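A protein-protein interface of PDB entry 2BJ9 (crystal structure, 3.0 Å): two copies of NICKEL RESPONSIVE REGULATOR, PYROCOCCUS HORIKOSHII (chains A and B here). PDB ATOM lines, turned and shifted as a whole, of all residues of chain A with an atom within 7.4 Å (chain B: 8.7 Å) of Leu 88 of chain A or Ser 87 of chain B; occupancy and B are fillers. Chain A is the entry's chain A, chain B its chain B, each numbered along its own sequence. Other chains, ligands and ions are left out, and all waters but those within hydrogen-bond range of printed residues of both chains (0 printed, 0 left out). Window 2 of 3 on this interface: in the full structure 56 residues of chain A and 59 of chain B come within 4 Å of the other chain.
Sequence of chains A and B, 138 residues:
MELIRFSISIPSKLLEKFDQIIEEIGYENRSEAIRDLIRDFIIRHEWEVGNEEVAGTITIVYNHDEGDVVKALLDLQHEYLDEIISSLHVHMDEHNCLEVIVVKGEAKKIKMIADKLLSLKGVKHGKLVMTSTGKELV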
ATOM      1  N   ILE A  58       0.959  15.249 -21.121  1.00  0.00           N
ATOM      2  CA  ILE A  58       1.381  13.901 -21.455  1.00  0.00           C
ATOM      3  C   ILE A  58       1.135  13.732 -22.945  1.00  0.00           C
ATOM      4  O   ILE A  58      -0.005  13.610 -23.376  1.00  0.00           O
ATOM      5  CB  ILE A  58       0.549  12.856 -20.716  1.00  0.00           C
ATOM      6  CG1 ILE A  58       0.671  13.063 -19.204  1.00  0.00           C
ATOM      7  CG2 ILE A  58       1.002  11.470 -21.123  1.00  0.00           C
ATOM      8  CD1 ILE A  58      -0.257  12.182 -18.406  1.00  0.00           C
ATOM      9  N   ILE A  60       1.202  11.582 -26.258  1.00  0.00           N
ATOM     10  CA  ILE A  60       1.258  10.176 -26.650  1.00  0.00           C
ATOM     11  C   ILE A  60       0.959   9.945 -28.122  1.00  0.00           C
ATOM     12  O   ILE A  60       0.287  10.743 -28.752  1.00  0.00           O
ATOM     13  CB  ILE A  60       0.300   9.300 -25.813  1.00  0.00           C
ATOM     14  CG1 ILE A  60      -1.137   9.743 -26.001  1.00  0.00           C
ATOM     15  CG2 ILE A  60       0.651   9.406 -24.347  1.00  0.00           C
ATOM     16  CD1 ILE A  60      -2.117   8.851 -25.260  1.00  0.00           C
ATOM     17  N   SER A  86      -7.941  18.522 -19.986  1.00  0.00           N
ATOM     18  CA  SER A  86      -8.388  18.344 -21.365  1.00  0.00           C
ATOM     19  C   SER A  86      -7.361  17.548 -22.152  1.00  0.00           C
ATOM     20  O   SER A  86      -6.292  17.217 -21.639  1.00  0.00           O
ATOM     21  CB  SER A  86      -8.569  19.696 -22.052  1.00  0.00           C
ATOM     22  OG  SER A  86      -9.584  20.446 -21.426  1.00  0.00           O
ATOM     23  N   SER A  87      -7.691  17.249 -23.404  1.00  0.00           N
ATOM     24  CA  SER A  87      -6.775  16.527 -24.265  1.00  0.00           C
ATOM     25  C   SER A  87      -6.973  16.935 -25.721  1.00  0.00           C
ATOM     26  O   SER A  87      -8.093  16.989 -26.215  1.00  0.00           O
ATOM     27  CB  SER A  87      -6.979  15.026 -24.117  1.00  0.00           C
ATOM     28  OG  SER A  87      -8.222  14.643 -24.649  1.00  0.00           O
ATOM     29  N   LEU A  88      -5.869  17.240 -26.395  1.00  0.00           N
ATOM     30  CA  LEU A  88      -5.880  17.629 -27.801  1.00  0.00           C
ATOM     31  C   LEU A  88      -5.484  16.399 -28.617  1.00  0.00           C
ATOM     32  O   LEU A  88      -4.462  15.776 -28.358  1.00  0.00           O
ATOM     33  CB  LEU A  88      -4.883  18.768 -28.023  1.00  0.00           C
ATOM     34  CG  LEU A  88      -4.732  19.308 -29.439  1.00  0.00           C
ATOM     35  CD1 LEU A  88      -6.107  19.556 -30.025  1.00  0.00           C
ATOM     36  CD2 LEU A  88      -3.927  20.590 -29.411  1.00  0.00           C
ATOM     37  N   HIS A  89      -6.299  16.048 -29.597  1.00  0.00           N
ATOM     38  CA  HIS A  89      -6.036  14.883 -30.424  1.00  0.00           C
ATOM     39  C   HIS A  89      -5.910  15.281 -31.886  1.00  0.00           C
ATOM     40  O   HIS A  89      -6.754  15.995 -32.419  1.00  0.00           O
ATOM     41  CB  HIS A  89      -7.167  13.873 -30.216  1.00  0.00           C
ATOM     42  CG  HIS A  89      -7.074  12.649 -31.075  1.00  0.00           C
ATOM     43  ND1 HIS A  89      -7.420  11.397 -30.613  1.00  0.00           N
ATOM     44  CD2 HIS A  89      -6.748  12.489 -32.380  1.00  0.00           C
ATOM     45  CE1 HIS A  89      -7.313  10.521 -31.595  1.00  0.00           C
ATOM     46  NE2 HIS A  89      -6.907  11.158 -32.678  1.00  0.00           N
ATOM     47  N   VAL A  90      -4.842  14.812 -32.523  1.00  0.00           N
ATOM     48  CA  VAL A  90      -4.557  15.091 -33.932  1.00  0.00           C
ATOM     49  C   VAL A  90      -4.415  13.783 -34.698  1.00  0.00           C
ATOM     50  O   VAL A  90      -3.521  12.997 -34.402  1.00  0.00           O
ATOM     51  CB  VAL A  90      -3.243  15.867 -34.075  1.00  0.00           C
ATOM     52  CG1 VAL A  90      -2.927  16.106 -35.547  1.00  0.00           C
ATOM     53  CG2 VAL A  90      -3.343  17.180 -33.312  1.00  0.00           C
ATOM     54  N   LEU A  98      -2.109  11.254 -32.432  1.00  0.00           N
ATOM     55  CA  LEU A  98      -1.177  11.900 -31.519  1.00  0.00           C
ATOM     56  C   LEU A  98      -2.099  12.634 -30.566  1.00  0.00           C
ATOM     57  O   LEU A  98      -2.975  13.382 -30.987  1.00  0.00           O
ATOM     58  CB  LEU A  98      -0.258  12.886 -32.235  1.00  0.00           C
ATOM     59  CG  LEU A  98       0.846  13.528 -31.379  1.00  0.00           C
ATOM     60  CD1 LEU A  98       1.804  14.297 -32.276  1.00  0.00           C
ATOM     61  CD2 LEU A  98       0.249  14.464 -30.332  1.00  0.00           C
ATOM     62  N   GLU A  99      -1.903  12.414 -29.278  1.00  0.00           N
ATOM     63  CA  GLU A  99      -2.746  13.027 -28.282  1.00  0.00           C
ATOM     64  C   GLU A  99      -1.901  13.715 -27.223  1.00  0.00           C
ATOM     65  O   GLU A  99      -0.878  13.181 -26.803  1.00  0.00           O
ATOM     66  CB  GLU A  99      -3.606  11.932 -27.655  1.00  0.00           C
ATOM     67  CG  GLU A  99      -4.760  12.403 -26.796  1.00  0.00           C
ATOM     68  CD  GLU A  99      -5.715  11.268 -26.446  1.00  0.00           C
ATOM     69  OE1 GLU A  99      -6.175  10.564 -27.378  1.00  0.00           O
ATOM     70  OE2 GLU A  99      -6.012  11.084 -25.244  1.00  0.00           O
ATOM     71  N   VAL A 100      -2.314  14.913 -26.824  1.00  0.00           N
ATOM     72  CA  VAL A 100      -1.626  15.650 -25.771  1.00  0.00           C
ATOM     73  C   VAL A 100      -2.651  15.812 -24.681  1.00  0.00           C
ATOM     74  O   VAL A 100      -3.759  16.250 -24.941  1.00  0.00           O
ATOM     75  CB  VAL A 100      -1.191  17.041 -26.192  1.00  0.00           C
ATOM     76  CG1 VAL A 100      -0.487  17.705 -25.037  1.00  0.00           C
ATOM     77  CG2 VAL A 100      -0.270  16.966 -27.375  1.00  0.00           C
ATOM     78  N   ILE A 101      -2.291  15.457 -23.460  1.00  0.00           N
ATOM     79  CA  ILE A 101      -3.221  15.546 -22.346  1.00  0.00           C
ATOM     80  C   ILE A 101      -2.690  16.522 -21.312  1.00  0.00           C
ATOM     81  O   ILE A 101      -1.576  16.357 -20.823  1.00  0.00           O
ATOM     82  CB  ILE A 101      -3.388  14.180 -21.711  1.00  0.00           C
ATOM     83  CG1 ILE A 101      -3.786  13.175 -22.793  1.00  0.00           C
ATOM     84  CG2 ILE A 101      -4.404  14.247 -20.604  1.00  0.00           C
ATOM     85  CD1 ILE A 101      -3.846  11.736 -22.331  1.00  0.00           C
ATOM     86  N   VAL A 102      -3.478  17.545 -20.988  1.00  0.00           N
ATOM     87  CA  VAL A 102      -3.049  18.535 -20.006  1.00  0.00           C
ATOM     88  C   VAL A 102      -3.538  18.119 -18.626  1.00  0.00           C
ATOM     89  O   VAL A 102      -4.703  17.779 -18.451  1.00  0.00           O
ATOM     90  CB  VAL A 102      -3.581  19.931 -20.357  1.00  0.00           C
ATOM     91  CG1 VAL A 102      -3.011  20.957 -19.401  1.00  0.00           C
ATOM     92  CG2 VAL A 102      -3.203  20.283 -21.789  1.00  0.00           C
ATOM     93  N   THR B  57       5.739  18.323 -29.442  1.00  0.00           N
ATOM     94  CA  THR B  57       4.835  19.183 -28.695  1.00  0.00           C
ATOM     95  C   THR B  57       5.577  20.078 -27.724  1.00  0.00           C
ATOM     96  O   THR B  57       6.135  19.619 -26.726  1.00  0.00           O
ATOM     97  CB  THR B  57       3.778  18.373 -27.924  1.00  0.00           C
ATOM     98  OG1 THR B  57       4.424  17.494 -27.001  1.00  0.00           O
ATOM     99  CG2 THR B  57       2.950  17.551 -28.875  1.00  0.00           C
ATOM    100  N   ILE B  58       5.565  21.368 -28.042  1.00  0.00           N
ATOM    101  CA  ILE B  58       6.206  22.415 -27.254  1.00  0.00           C
ATOM    102  C   ILE B  58       5.253  22.863 -26.145  1.00  0.00           C
ATOM    103  O   ILE B  58       4.208  23.450 -26.412  1.00  0.00           O
ATOM    104  CB  ILE B  58       6.544  23.621 -28.167  1.00  0.00           C
ATOM    105  CG1 ILE B  58       7.496  23.167 -29.272  1.00  0.00           C
ATOM    106  CG2 ILE B  58       7.134  24.759 -27.356  1.00  0.00           C
ATOM    107  CD1 ILE B  58       7.813  24.219 -30.281  1.00  0.00           C
ATOM    108  N   ILE B  60       4.587  25.203 -22.906  1.00  0.00           N
ATOM    109  CA  ILE B  60       5.099  26.415 -22.283  1.00  0.00           C
ATOM    110  C   ILE B  60       4.149  26.987 -21.254  1.00  0.00           C
ATOM    111  O   ILE B  60       2.936  26.774 -21.317  1.00  0.00           O
ATOM    112  CB  ILE B  60       5.383  27.513 -23.319  1.00  0.00           C
ATOM    113  CG1 ILE B  60       4.112  27.842 -24.098  1.00  0.00           C
ATOM    114  CG2 ILE B  60       6.474  27.058 -24.271  1.00  0.00           C
ATOM    115  CD1 ILE B  60       4.315  28.887 -25.188  1.00  0.00           C
ATOM    116  N   TYR B  62       3.465  30.721 -19.074  1.00  0.00           N
ATOM    117  CA  TYR B  62       3.791  32.141 -19.033  1.00  0.00           C
ATOM    118  C   TYR B  62       2.683  32.977 -18.399  1.00  0.00           C
ATOM    119  O   TYR B  62       1.589  32.483 -18.132  1.00  0.00           O
ATOM    120  CB  TYR B  62       4.054  32.639 -20.459  1.00  0.00           C
ATOM    121  CG  TYR B  62       2.861  32.470 -21.376  1.00  0.00           C
ATOM    122  CD1 TYR B  62       1.747  33.288 -21.262  1.00  0.00           C
ATOM    123  CD2 TYR B  62       2.829  31.457 -22.326  1.00  0.00           C
ATOM    124  CE1 TYR B  62       0.633  33.100 -22.061  1.00  0.00           C
ATOM    125  CE2 TYR B  62       1.715  31.260 -23.134  1.00  0.00           C
ATOM    126  CZ  TYR B  62       0.618  32.083 -22.994  1.00  0.00           C
ATOM    127  OH  TYR B  62      -0.508  31.874 -23.763  1.00  0.00           O
ATOM    128  N   LEU B  74       2.204  34.613 -30.661  1.00  0.00           N
ATOM    129  CA  LEU B  74       1.359  34.437 -31.842  1.00  0.00           C
ATOM    130  C   LEU B  74       2.099  34.733 -33.140  1.00  0.00           C
ATOM    131  O   LEU B  74       2.077  33.923 -34.064  1.00  0.00           O
ATOM    132  CB  LEU B  74       0.116  35.316 -31.745  1.00  0.00           C
ATOM    133  CG  LEU B  74      -0.932  34.867 -30.728  1.00  0.00           C
ATOM    134  CD1 LEU B  74      -2.021  35.913 -30.625  1.00  0.00           C
ATOM    135  CD2 LEU B  74      -1.513  33.529 -31.147  1.00  0.00           C
ATOM    136  N   GLN B  77       4.408  31.988 -33.862  1.00  0.00           N
ATOM    137  CA  GLN B  77       3.621  30.841 -34.277  1.00  0.00           C
ATOM    138  C   GLN B  77       3.014  31.019 -35.659  1.00  0.00           C
ATOM    139  O   GLN B  77       3.036  30.100 -36.468  1.00  0.00           O
ATOM    140  CB  GLN B  77       2.517  30.564 -33.256  1.00  0.00           C
ATOM    141  CG  GLN B  77       3.036  30.212 -31.866  1.00  0.00           C
ATOM    142  CD  GLN B  77       1.957  29.656 -30.960  1.00  0.00           C
ATOM    143  OE1 GLN B  77       1.383  28.601 -31.234  1.00  0.00           O
ATOM    144  NE2 GLN B  77       1.674  30.366 -29.873  1.00  0.00           N
ATOM    145  N   ILE B  84       2.980  24.186 -37.498  1.00  0.00           N
ATOM    146  CA  ILE B  84       2.083  24.154 -36.346  1.00  0.00           C
ATOM    147  C   ILE B  84       0.696  23.670 -36.744  1.00  0.00           C
ATOM    148  O   ILE B  84       0.106  24.175 -37.690  1.00  0.00           O
ATOM    149  CB  ILE B  84       1.954  25.537 -35.711  1.00  0.00           C
ATOM    150  CG1 ILE B  84       3.316  25.993 -35.184  1.00  0.00           C
ATOM    151  CG2 ILE B  84       0.921  25.496 -34.614  1.00  0.00           C
ATOM    152  CD1 ILE B  84       3.299  27.352 -34.566  1.00  0.00           C
ATOM    153  N   ILE B  85       0.176  22.692 -36.014  1.00  0.00           N
ATOM    154  CA  ILE B  85      -1.137  22.134 -36.310  1.00  0.00           C
ATOM    155  C   ILE B  85      -2.213  22.886 -35.556  1.00  0.00           C
ATOM    156  O   ILE B  85      -3.177  23.364 -36.142  1.00  0.00           O
ATOM    157  CB  ILE B  85      -1.188  20.655 -35.919  1.00  0.00           C
ATOM    158  CG1 ILE B  85      -0.154  19.883 -36.729  1.00  0.00           C
ATOM    159  CG2 ILE B  85      -2.581  20.096 -36.128  1.00  0.00           C
ATOM    160  CD1 ILE B  85      -0.088  18.429 -36.361  1.00  0.00           C
ATOM    161  N   SER B  86      -2.032  22.984 -34.246  1.00  0.00           N
ATOM    162  CA  SER B  86      -2.963  23.693 -33.376  1.00  0.00           C
ATOM    163  C   SER B  86      -2.408  23.623 -31.967  1.00  0.00           C
ATOM    164  O   SER B  86      -1.611  22.743 -31.661  1.00  0.00           O
ATOM    165  CB  SER B  86      -4.352  23.052 -33.425  1.00  0.00           C
ATOM    166  OG  SER B  86      -4.297  21.709 -33.010  1.00  0.00           O
ATOM    167  N   SER B  87      -2.804  24.560 -31.118  1.00  0.00           N
ATOM    168  CA  SER B  87      -2.325  24.556 -29.748  1.00  0.00           C
ATOM    169  C   SER B  87      -3.494  24.491 -28.790  1.00  0.00           C
ATOM    170  O   SER B  87      -4.599  24.913 -29.121  1.00  0.00           O
ATOM    171  CB  SER B  87      -1.530  25.819 -29.457  1.00  0.00           C
ATOM    172  OG  SER B  87      -2.404  26.911 -29.240  1.00  0.00           O
ATOM    173  N   LEU B  88      -3.247  23.949 -27.601  1.00  0.00           N
ATOM    174  CA  LEU B  88      -4.265  23.860 -26.563  1.00  0.00           C
ATOM    175  C   LEU B  88      -3.833  24.836 -25.472  1.00  0.00           C
ATOM    176  O   LEU B  88      -2.641  24.983 -25.199  1.00  0.00           O
ATOM    177  CB  LEU B  88      -4.345  22.439 -26.023  1.00  0.00           C
ATOM    178  CG  LEU B  88      -5.439  22.158 -25.001  1.00  0.00           C
ATOM    179  CD1 LEU B  88      -5.651  20.661 -24.867  1.00  0.00           C
ATOM    180  CD2 LEU B  88      -5.042  22.754 -23.683  1.00  0.00           C
ATOM    181  N   HIS B  89      -4.797  25.512 -24.861  1.00  0.00           N
ATOM    182  CA  HIS B  89      -4.495  26.500 -23.829  1.00  0.00           C
ATOM    183  C   HIS B  89      -5.370  26.331 -22.598  1.00  0.00           C
ATOM    184  O   HIS B  89      -6.584  26.150 -22.700  1.00  0.00           O
ATOM    185  CB  HIS B  89      -4.667  27.908 -24.407  1.00  0.00           C
ATOM    186  CG  HIS B  89      -4.333  29.009 -23.451  1.00  0.00           C
ATOM    187  ND1 HIS B  89      -3.574  30.100 -23.818  1.00  0.00           N
ATOM    188  CD2 HIS B  89      -4.690  29.217 -22.163  1.00  0.00           C
ATOM    189  CE1 HIS B  89      -3.480  30.934 -22.799  1.00  0.00           C
ATOM    190  NE2 HIS B  89      -4.148  30.421 -21.781  1.00  0.00           N
ATOM    191  N   VAL B  90      -4.728  26.378 -21.435  1.00  0.00           N
ATOM    192  CA  VAL B  90      -5.408  26.248 -20.152  1.00  0.00           C
ATOM    193  C   VAL B  90      -5.032  27.443 -19.295  1.00  0.00           C
ATOM    194  O   VAL B  90      -3.857  27.792 -19.214  1.00  0.00           O
ATOM    195  CB  VAL B  90      -4.968  24.976 -19.408  1.00  0.00           C
ATOM    196  CG1 VAL B  90      -5.575  24.948 -18.030  1.00  0.00           C
ATOM    197  CG2 VAL B  90      -5.396  23.749 -20.174  1.00  0.00           C
ATOM    198  N   LEU B  98      -1.058  28.051 -19.438  1.00  0.00           N
ATOM    199  CA  LEU B  98      -0.271  26.887 -19.830  1.00  0.00           C
ATOM    200  C   LEU B  98      -0.691  26.602 -21.268  1.00  0.00           C
ATOM    201  O   LEU B  98      -1.877  26.470 -21.559  1.00  0.00           O
ATOM    202  CB  LEU B  98      -0.590  25.685 -18.938  1.00  0.00           C
ATOM    203  CG  LEU B  98       0.178  24.387 -19.209  1.00  0.00           C
ATOM    204  CD1 LEU B  98      -0.080  23.386 -18.108  1.00  0.00           C
ATOM    205  CD2 LEU B  98      -0.260  23.806 -20.524  1.00  0.00           C
ATOM    206  N   GLU B  99       0.273  26.512 -22.170  1.00  0.00           N
ATOM    207  CA  GLU B  99      -0.058  26.268 -23.561  1.00  0.00           C
ATOM    208  C   GLU B  99       0.777  25.111 -24.095  1.00  0.00           C
ATOM    209  O   GLU B  99       1.947  24.988 -23.752  1.00  0.00           O
ATOM    210  CB  GLU B  99       0.209  27.543 -24.371  1.00  0.00           C
ATOM    211  CG  GLU B  99      -0.572  27.667 -25.664  1.00  0.00           C
ATOM    212  CD  GLU B  99      -0.466  29.055 -26.285  1.00  0.00           C
ATOM    213  OE1 GLU B  99      -0.660  30.045 -25.549  1.00  0.00           O
ATOM    214  OE2 GLU B  99      -0.202  29.159 -27.504  1.00  0.00           O
ATOM    215  N   VAL B 100       0.171  24.256 -24.912  1.00  0.00           N
ATOM    216  CA  VAL B 100       0.894  23.138 -25.504  1.00  0.00           C
ATOM    217  C   VAL B 100       0.700  23.135 -27.022  1.00  0.00           C
ATOM    218  O   VAL B 100      -0.359  22.790 -27.523  1.00  0.00           O
ATOM    219  CB  VAL B 100       0.439  21.783 -24.909  1.00  0.00           C
ATOM    220  CG1 VAL B 100      -1.058  21.676 -24.932  1.00  0.00           C
ATOM    221  CG2 VAL B 100       1.049  20.646 -25.694  1.00  0.00           C
ATOM    222  N   ILE B 101       1.737  23.534 -27.748  1.00  0.00           N
ATOM    223  CA  ILE B 101       1.691  23.589 -29.208  1.00  0.00           C
ATOM    224  C   ILE B 101       2.040  22.239 -29.844  1.00  0.00           C
ATOM    225  O   ILE B 101       2.981  21.565 -29.421  1.00  0.00           O
ATOM    226  CB  ILE B 101       2.680  24.633 -29.723  1.00  0.00           C
ATOM    227  CG1 ILE B 101       2.623  25.866 -28.818  1.00  0.00           C
ATOM    228  CG2 ILE B 101       2.366  24.977 -31.171  1.00  0.00           C
ATOM    229  CD1 ILE B 101       3.532  26.987 -29.242  1.00  0.00           C
ATOM    230  N   VAL B 102       1.292  21.846 -30.867  1.00  0.00           N
ATOM    231  CA  VAL B 102       1.538  20.573 -31.542  1.00  0.00           C
ATOM    232  C   VAL B 102       2.123  20.852 -32.914  1.00  0.00           C
ATOM    233  O   VAL B 102       1.510  21.538 -33.724  1.00  0.00           O
ATOM    234  CB  VAL B 102       0.230  19.770 -31.668  1.00  0.00           C
ATOM    235  CG1 VAL B 102       0.434  18.523 -32.500  1.00  0.00           C
ATOM    236  CG2 VAL B 102      -0.248  19.404 -30.291  1.00  0.00           C
ATOM    237  N   VAL B 103       3.309  20.313 -33.175  1.00  0.00           N
ATOM    238  CA  VAL B 103       3.990  20.554 -34.442  1.00  0.00           C
ATOM    239  C   VAL B 103       4.265  19.306 -35.271  1.00  0.00           C
ATOM    240  O   VAL B 103       4.459  18.217 -34.734  1.00  0.00           O
ATOM    241  CB  VAL B 103       5.329  21.239 -34.206  1.00  0.00           C
ATOM    242  CG1 VAL B 103       5.763  21.942 -35.460  1.00  0.00           C
ATOM    243  CG2 VAL B 103       5.229  22.198 -33.052  1.00  0.00           C
ATOM    244  N   LEU B 117      10.550  30.021 -29.407  1.00  0.00           N
ATOM    245  CA  LEU B 117       9.514  30.174 -28.395  1.00  0.00           C
ATOM    246  C   LEU B 117      10.046  30.128 -26.987  1.00  0.00           C
ATOM    247  O   LEU B 117       9.810  31.039 -26.198  1.00  0.00           O
ATOM    248  CB  LEU B 117       8.434  29.100 -28.539  1.00  0.00           C
ATOM    249  CG  LEU B 117       7.603  29.092 -29.825  1.00  0.00           C
ATOM    250  CD1 LEU B 117       6.546  28.015 -29.736  1.00  0.00           C
ATOM    251  CD2 LEU B 117       6.962  30.446 -30.034  1.00  0.00           C
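N of Ile 85 of chain B lies within hydrogen-bond range of O of Val 102 of chain B, 2.9 Å away.
The backbone carbonyl oxygen of Ser 86 of chain B is in hydrogen-bond range of the backbone NH of Val 102 of chain B (3.1 Å).
The backbone carbonyl oxygen (O) of Ser 86 of chain A is in hydrogen-bond range of the backbone NH (N) of Val 102 of chain A.
The backbone NH (N) of Leu 98 of chain B lies within hydrogen-bond range of the backbone carbonyl oxygen (O) of Val 90 of chain B, at 2.8 Å.
The backbone NH (N) of Val 100 of chain B lies within hydrogen-bond range of the backbone carbonyl oxygen (O) of Leu 88 of chain B (2.9 Å).
The backbone NH of Leu 88 of chain A is in hydrogen-bond range of the backbone carbonyl oxygen of Val 100 of chain A (2.7 Å).
Among the printed residues, merely in contact across the chains: Val 100 of chain A with Val 100 of chain B, Val 100 of chain A with Thr 57 of chain B, Val 102 of chain A with Leu 88 of chain B, Val 102 of chain A with Val 90 of chain B, Leu 88 of chain A with Leu 88 of chain B, Val 90 of chain A with Ile 85 of chain B, Leu 88 of chain A with Ser 86 of chain B, Val 100 of chain A with Val 102 of chain B, Leu 88 of chain A with Val 102 of chain B and Leu 88 of chain A with Ser 87 of chain B.
Of chain B, only Ser 86, Ser 87, Leu 88 and Val 102 come within 4 Å of Leu 88 of chain A.
Printed residues of chain A within 4 Å of Ser 87 of chain B: Leu 88.
No residue of chain B comes within 4 Å of Ser 87 of chain A.
Of the printed residues of chain A, Val 90 of chain B touches Val 102.
Of the printed residues of chain A, Val 102 of chain B touches Leu 88 and Val 100.
Printed residues of chain A within 4 Å of Leu 88 of chain B: Leu 88 (3.8 Å) and Val 102 (3.6 Å).
Of the printed residues of chain B, Val 90 of chain A touches Ile 85 (3.8 Å).
Glu 99 of chain A touches none of the printed residues of chain B.
Leu 98 of chain B touches none of the printed residues of chain A.
The nearest printed residue of chain A that does not touch Ser 87 of chain B is Val 90 of chain A (7.7 Å).
Hydrophobic or aromatic side chains of chain A within 4 Å of the printed part of chain B: Leu 88, Val 90, Val 100 and Val 102.
Along chain B the printed residues that touch a printed residue of chain A span positions 57 to 102.
Among the printed residues, 10 pairs touch across the chains.
Leu 88 of chain A touches Ser 86 of chain B, but with the chains exchanged Ser 86 of chain A does not touch Leu 88 of chain B (4.2 Å).
Leu 88 of chain A touches Ser 87 of chain B, but with the chains exchanged Ser 87 of chain A does not touch Leu 88 of chain B (4.04 Å).
Leu 88 of chain A touches Val 102 of chain B, and with the chains exchanged Val 102 of chain A touches Leu 88 of chain B.
Val 102 of chain A touches Val 90 of chain B, but with the chains exchanged Val 90 of chain A does not touch Val 102 of chain B (4.1 Å).
Positions printed for both chains: 58, 60, 86, 87, 88, 89, 90, 98, 99, 100, 101 and 102.
Of the 10 pairs that touch across the chains among the printed residues, 4 have their exchanged pair printed and touching as well.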
